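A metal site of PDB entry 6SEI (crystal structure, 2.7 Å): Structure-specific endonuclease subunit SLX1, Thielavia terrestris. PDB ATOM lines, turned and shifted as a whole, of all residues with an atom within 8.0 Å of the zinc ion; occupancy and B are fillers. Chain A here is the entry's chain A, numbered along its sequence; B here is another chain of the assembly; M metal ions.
Within 4 Å of the zinc ion: Cys 229, Cys 232, His 256 and Cys 259.
The zinc ion is bound by ND1 of His 256.
SG of Cys 232 is bound to the zinc ion (2.3 Å).
The zinc ion is bound by SG of Cys 229 (2.4 Å).
The zinc ion is bound by the side-chain sulfur (SG) of Cys 259 (2.6 Å).
The zinc ion has four donor atoms within binding distance.
A ring nitrogen (NE2) of His 256 lies within hydrogen-bond range of the guanidinium group (NH2) of Arg 32 of chain B.
The side-chain sulfur of Cys 259 lies close to the guanidinium group of Arg 262, 3.3 Å away.
SG of Cys 229 sits close to N of Val 231 (3.5 Å).
The backbone NH (N) of Glu 234 sits close to the side-chain sulfur (SG) of Cys 232 (3.6 Å).
The side-chain sulfur (SD) of Met 236 lies close to the backbone NH (N) of Cys 229 (3.7 Å).
The backbone carbonyl oxygen (O) of Glu 234 lies within hydrogen-bond range of the backbone NH (N) of Cys 229 (3.0 Å).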
ATOM      1  N   ALA A 228     -14.861   4.169  13.130  1.00  0.00           N
ATOM      2  CA  ALA A 228     -15.194   5.576  12.927  1.00  0.00           C
ATOM      3  C   ALA A 228     -15.164   6.319  14.257  1.00  0.00           C
ATOM      4  O   ALA A 228     -15.323   5.739  15.333  1.00  0.00           O
ATOM      5  CB  ALA A 228     -16.574   5.731  12.268  1.00  0.00           C
ATOM      6  N   CYS A 229     -14.936   7.622  14.166  1.00  0.00           N
ATOM      7  CA  CYS A 229     -14.814   8.464  15.343  1.00  0.00           C
ATOM      8  C   CYS A 229     -16.098   8.444  16.167  1.00  0.00           C
ATOM      9  O   CYS A 229     -17.187   8.714  15.649  1.00  0.00           O
ATOM     10  CB  CYS A 229     -14.473   9.887  14.914  1.00  0.00           C
ATOM     11  SG  CYS A 229     -14.401  11.111  16.229  1.00  0.00           S
ATOM     12  N   VAL A 230     -15.953   8.139  17.451  1.00  0.00           N
ATOM     13  CA  VAL A 230     -17.085   8.028  18.349  1.00  0.00           C
ATOM     14  C   VAL A 230     -17.808   9.346  18.547  1.00  0.00           C
ATOM     15  O   VAL A 230     -18.928   9.358  19.065  1.00  0.00           O
ATOM     16  CB  VAL A 230     -16.666   7.455  19.718  1.00  0.00           C
ATOM     17  CG1 VAL A 230     -16.339   5.979  19.606  1.00  0.00           C
ATOM     18  CG2 VAL A 230     -15.478   8.229  20.267  1.00  0.00           C
ATOM     19  N   VAL A 231     -17.202  10.462  18.150  1.00  0.00           N
ATOM     20  CA  VAL A 231     -17.813  11.774  18.323  1.00  0.00           C
ATOM     21  C   VAL A 231     -18.483  12.224  17.034  1.00  0.00           C
ATOM     22  O   VAL A 231     -19.712  12.402  16.992  1.00  0.00           O
ATOM     23  CB  VAL A 231     -16.775  12.805  18.811  1.00  0.00           C
ATOM     24  CG1 VAL A 231     -17.471  14.058  19.323  1.00  0.00           C
ATOM     25  CG2 VAL A 231     -15.890  12.205  19.899  1.00  0.00           C
ATOM     26  N   CYS A 232     -17.704  12.405  15.957  1.00  0.00           N
ATOM     27  CA  CYS A 232     -18.202  12.991  14.717  1.00  0.00           C
ATOM     28  C   CYS A 232     -18.789  11.962  13.744  1.00  0.00           C
ATOM     29  O   CYS A 232     -19.351  12.360  12.722  1.00  0.00           O
ATOM     30  CB  CYS A 232     -17.078  13.782  14.028  1.00  0.00           C
ATOM     31  SG  CYS A 232     -15.851  12.828  13.150  1.00  0.00           S
ATOM     32  N   ARG A 233     -18.662  10.664  14.042  1.00  0.00           N
ATOM     33  CA  ARG A 233     -19.206   9.551  13.254  1.00  0.00           C
ATOM     34  C   ARG A 233     -18.550   9.383  11.887  1.00  0.00           C
ATOM     35  O   ARG A 233     -19.083   8.670  11.035  1.00  0.00           O
ATOM     36  CB  ARG A 233     -20.727   9.679  13.059  1.00  0.00           C
ATOM     37  CG  ARG A 233     -21.525   9.978  14.313  1.00  0.00           C
ATOM     38  CD  ARG A 233     -22.986   9.627  14.118  1.00  0.00           C
ATOM     39  NE  ARG A 233     -23.595  10.397  13.028  1.00  0.00           N
ATOM     40  CZ  ARG A 233     -24.732  10.072  12.433  1.00  0.00           C
ATOM     41  NH1 ARG A 233     -25.398   8.984  12.807  1.00  0.00           N
ATOM     42  NH2 ARG A 233     -25.216  10.822  11.452  1.00  0.00           N
ATOM     43  N   GLU A 234     -17.397  10.002  11.653  1.00  0.00           N
ATOM     44  CA  GLU A 234     -16.722   9.907  10.359  1.00  0.00           C
ATOM     45  C   GLU A 234     -15.706   8.770  10.375  1.00  0.00           C
ATOM     46  O   GLU A 234     -14.966   8.592  11.347  1.00  0.00           O
ATOM     47  CB  GLU A 234     -16.025  11.221  10.024  1.00  0.00           C
ATOM     48  CG  GLU A 234     -15.049  11.129   8.859  1.00  0.00           C
ATOM     49  CD  GLU A 234     -14.239  12.398   8.665  1.00  0.00           C
ATOM     50  OE1 GLU A 234     -14.524  13.402   9.357  1.00  0.00           O
ATOM     51  OE2 GLU A 234     -13.319  12.397   7.826  1.00  0.00           O
ATOM     52  N   GLU A 235     -15.686   7.989   9.298  1.00  0.00           N
ATOM     53  CA  GLU A 235     -14.705   6.921   9.153  1.00  0.00           C
ATOM     54  C   GLU A 235     -13.290   7.466   9.310  1.00  0.00           C
ATOM     55  O   GLU A 235     -12.990   8.601   8.945  1.00  0.00           O
ATOM     56  CB  GLU A 235     -14.862   6.237   7.799  1.00  0.00           C
ATOM     57  CG  GLU A 235     -14.478   7.105   6.604  1.00  0.00           C
ATOM     58  CD  GLU A 235     -15.625   7.942   6.071  1.00  0.00           C
ATOM     59  OE1 GLU A 235     -16.703   7.971   6.715  1.00  0.00           O
ATOM     60  OE2 GLU A 235     -15.461   8.563   5.001  1.00  0.00           O
ATOM     61  N   MET A 236     -12.414   6.632   9.888  1.00  0.00           N
ATOM     62  CA  MET A 236     -11.013   7.019  10.135  1.00  0.00           C
ATOM     63  C   MET A 236     -10.112   5.986   9.469  1.00  0.00           C
ATOM     64  O   MET A 236      -9.811   4.946  10.053  1.00  0.00           O
ATOM     65  CB  MET A 236     -10.734   7.124  11.629  1.00  0.00           C
ATOM     66  CG  MET A 236     -11.710   8.017  12.383  1.00  0.00           C
ATOM     67  SD  MET A 236     -11.259   8.161  14.117  1.00  0.00           S
ATOM     68  CE  MET A 236     -11.731   6.533  14.674  1.00  0.00           C
ATOM     69  N   LEU A 242      -4.441  12.337  13.645  1.00  0.00           N
ATOM     70  CA  LEU A 242      -4.219  11.780  14.973  1.00  0.00           C
ATOM     71  C   LEU A 242      -5.530  11.205  15.496  1.00  0.00           C
ATOM     72  O   LEU A 242      -6.564  11.889  15.494  1.00  0.00           O
ATOM     73  CB  LEU A 242      -3.675  12.830  15.930  1.00  0.00           C
ATOM     74  CG  LEU A 242      -2.276  13.332  15.548  1.00  0.00           C
ATOM     75  CD1 LEU A 242      -2.169  14.829  15.773  1.00  0.00           C
ATOM     76  CD2 LEU A 242      -1.222  12.574  16.335  1.00  0.00           C
ATOM     77  N   VAL A 254     -12.242   4.982  19.402  1.00  0.00           N
ATOM     78  CA  VAL A 254     -11.225   5.811  18.764  1.00  0.00           C
ATOM     79  C   VAL A 254     -11.904   7.050  18.191  1.00  0.00           C
ATOM     80  O   VAL A 254     -13.023   6.980  17.676  1.00  0.00           O
ATOM     81  CB  VAL A 254     -10.466   5.060  17.646  1.00  0.00           C
ATOM     82  CG1 VAL A 254      -9.199   5.812  17.272  1.00  0.00           C
ATOM     83  CG2 VAL A 254     -10.132   3.645  18.086  1.00  0.00           C
ATOM     84  N   GLY A 255     -11.232   8.197  18.308  1.00  0.00           N
ATOM     85  CA  GLY A 255     -11.792   9.439  17.825  1.00  0.00           C
ATOM     86  C   GLY A 255     -10.709  10.349  17.266  1.00  0.00           C
ATOM     87  O   GLY A 255      -9.516  10.142  17.493  1.00  0.00           O
ATOM     88  N   HIS A 256     -11.164  11.345  16.510  1.00  0.00           N
ATOM     89  CA  HIS A 256     -10.247  12.390  16.065  1.00  0.00           C
ATOM     90  C   HIS A 256      -9.803  13.199  17.274  1.00  0.00           C
ATOM     91  O   HIS A 256     -10.614  13.553  18.134  1.00  0.00           O
ATOM     92  CB  HIS A 256     -10.934  13.296  15.043  1.00  0.00           C
ATOM     93  CG  HIS A 256     -11.243  12.610  13.749  1.00  0.00           C
ATOM     94  ND1 HIS A 256     -12.512  12.186  13.417  1.00  0.00           N
ATOM     95  CD2 HIS A 256     -10.452  12.280  12.695  1.00  0.00           C
ATOM     96  CE1 HIS A 256     -12.492  11.614  12.225  1.00  0.00           C
ATOM     97  NE2 HIS A 256     -11.253  11.655  11.766  1.00  0.00           N
ATOM     98  N   LEU A 257      -8.496  13.485  17.337  1.00  0.00           N
ATOM     99  CA  LEU A 257      -7.928  14.120  18.526  1.00  0.00           C
ATOM    100  C   LEU A 257      -8.696  15.365  18.912  1.00  0.00           C
ATOM    101  O   LEU A 257      -9.041  15.565  20.077  1.00  0.00           O
ATOM    102  CB  LEU A 257      -6.454  14.447  18.288  1.00  0.00           C
ATOM    103  CG  LEU A 257      -5.856  15.337  19.371  1.00  0.00           C
ATOM    104  CD1 LEU A 257      -5.883  14.607  20.716  1.00  0.00           C
ATOM    105  CD2 LEU A 257      -4.438  15.765  19.033  1.00  0.00           C
ATOM    106  N   SER A 258      -8.976  16.225  17.926  1.00  0.00           N
ATOM    107  CA  SER A 258      -9.730  17.443  18.177  1.00  0.00           C
ATOM    108  C   SER A 258     -11.233  17.205  18.324  1.00  0.00           C
ATOM    109  O   SER A 258     -11.944  18.130  18.720  1.00  0.00           O
ATOM    110  CB  SER A 258      -9.479  18.467  17.063  1.00  0.00           C
ATOM    111  OG  SER A 258      -9.784  17.932  15.791  1.00  0.00           O
ATOM    112  N   CYS A 259     -11.725  16.006  18.035  1.00  0.00           N
ATOM    113  CA  CYS A 259     -13.118  15.734  18.373  1.00  0.00           C
ATOM    114  C   CYS A 259     -13.230  15.329  19.850  1.00  0.00           C
ATOM    115  O   CYS A 259     -14.124  15.808  20.556  1.00  0.00           O
ATOM    116  CB  CYS A 259     -13.706  14.684  17.440  1.00  0.00           C
ATOM    117  SG  CYS A 259     -14.059  15.304  15.764  1.00  0.00           S
ATOM    118  N   TRP A 260     -12.316  14.476  20.334  1.00  0.00           N
ATOM    119  CA  TRP A 260     -12.292  14.114  21.746  1.00  0.00           C
ATOM    120  C   TRP A 260     -12.296  15.350  22.628  1.00  0.00           C
ATOM    121  O   TRP A 260     -13.120  15.488  23.534  1.00  0.00           O
ATOM    122  CB  TRP A 260     -11.057  13.263  22.058  1.00  0.00           C
ATOM    123  CG  TRP A 260     -11.222  11.782  21.855  1.00  0.00           C
ATOM    124  CD1 TRP A 260     -10.487  10.990  21.032  1.00  0.00           C
ATOM    125  CD2 TRP A 260     -12.132  10.899  22.543  1.00  0.00           C
ATOM    126  NE1 TRP A 260     -10.891   9.687  21.123  1.00  0.00           N
ATOM    127  CE2 TRP A 260     -11.892   9.601  22.042  1.00  0.00           C
ATOM    128  CE3 TRP A 260     -13.119  11.084  23.509  1.00  0.00           C
ATOM    129  CZ2 TRP A 260     -12.616   8.493  22.485  1.00  0.00           C
ATOM    130  CZ3 TRP A 260     -13.832   9.991  23.940  1.00  0.00           C
ATOM    131  CH2 TRP A 260     -13.580   8.708  23.427  1.00  0.00           C
ATOM    132  N   ARG A 262     -13.045  18.592  21.975  1.00  0.00           N
ATOM    133  CA  ARG A 262     -14.314  19.311  21.870  1.00  0.00           C
ATOM    134  C   ARG A 262     -15.422  18.598  22.644  1.00  0.00           C
ATOM    135  O   ARG A 262     -16.284  19.248  23.227  1.00  0.00           O
ATOM    136  CB  ARG A 262     -14.697  19.453  20.398  1.00  0.00           C
ATOM    137  CG  ARG A 262     -16.058  20.085  20.151  1.00  0.00           C
ATOM    138  CD  ARG A 262     -16.331  20.251  18.664  1.00  0.00           C
ATOM    139  NE  ARG A 262     -16.827  19.019  18.037  1.00  0.00           N
ATOM    140  CZ  ARG A 262     -16.124  18.286  17.182  1.00  0.00           C
ATOM    141  NH1 ARG A 262     -16.647  17.182  16.659  1.00  0.00           N
ATOM    142  NH2 ARG A 262     -14.883  18.657  16.846  1.00  0.00           N
ATOM    143  N   ARG B  32      -7.373  20.238  10.713  1.00  0.00           N
ATOM    144  CA  ARG B  32      -6.582  19.310  11.497  1.00  0.00           C
ATOM    145  C   ARG B  32      -5.530  18.617  10.631  1.00  0.00           C
ATOM    146  O   ARG B  32      -5.616  18.614   9.398  1.00  0.00           O
ATOM    147  CB  ARG B  32      -7.489  18.265  12.162  1.00  0.00           C
ATOM    148  CG  ARG B  32      -7.918  17.152  11.222  1.00  0.00           C
ATOM    149  CD  ARG B  32      -9.221  16.503  11.661  1.00  0.00           C
ATOM    150  NE  ARG B  32      -9.675  15.541  10.666  1.00  0.00           N
ATOM    151  CZ  ARG B  32     -10.940  15.139  10.535  1.00  0.00           C
ATOM    152  NH1 ARG B  32     -11.879  15.601  11.342  1.00  0.00           N
ATOM    153  NH2 ARG B  32     -11.256  14.266   9.588  1.00  0.00           N
HETATM  154 ZN    ZN M   1     -14.190  12.955  14.711  1.00  0.00          ZN
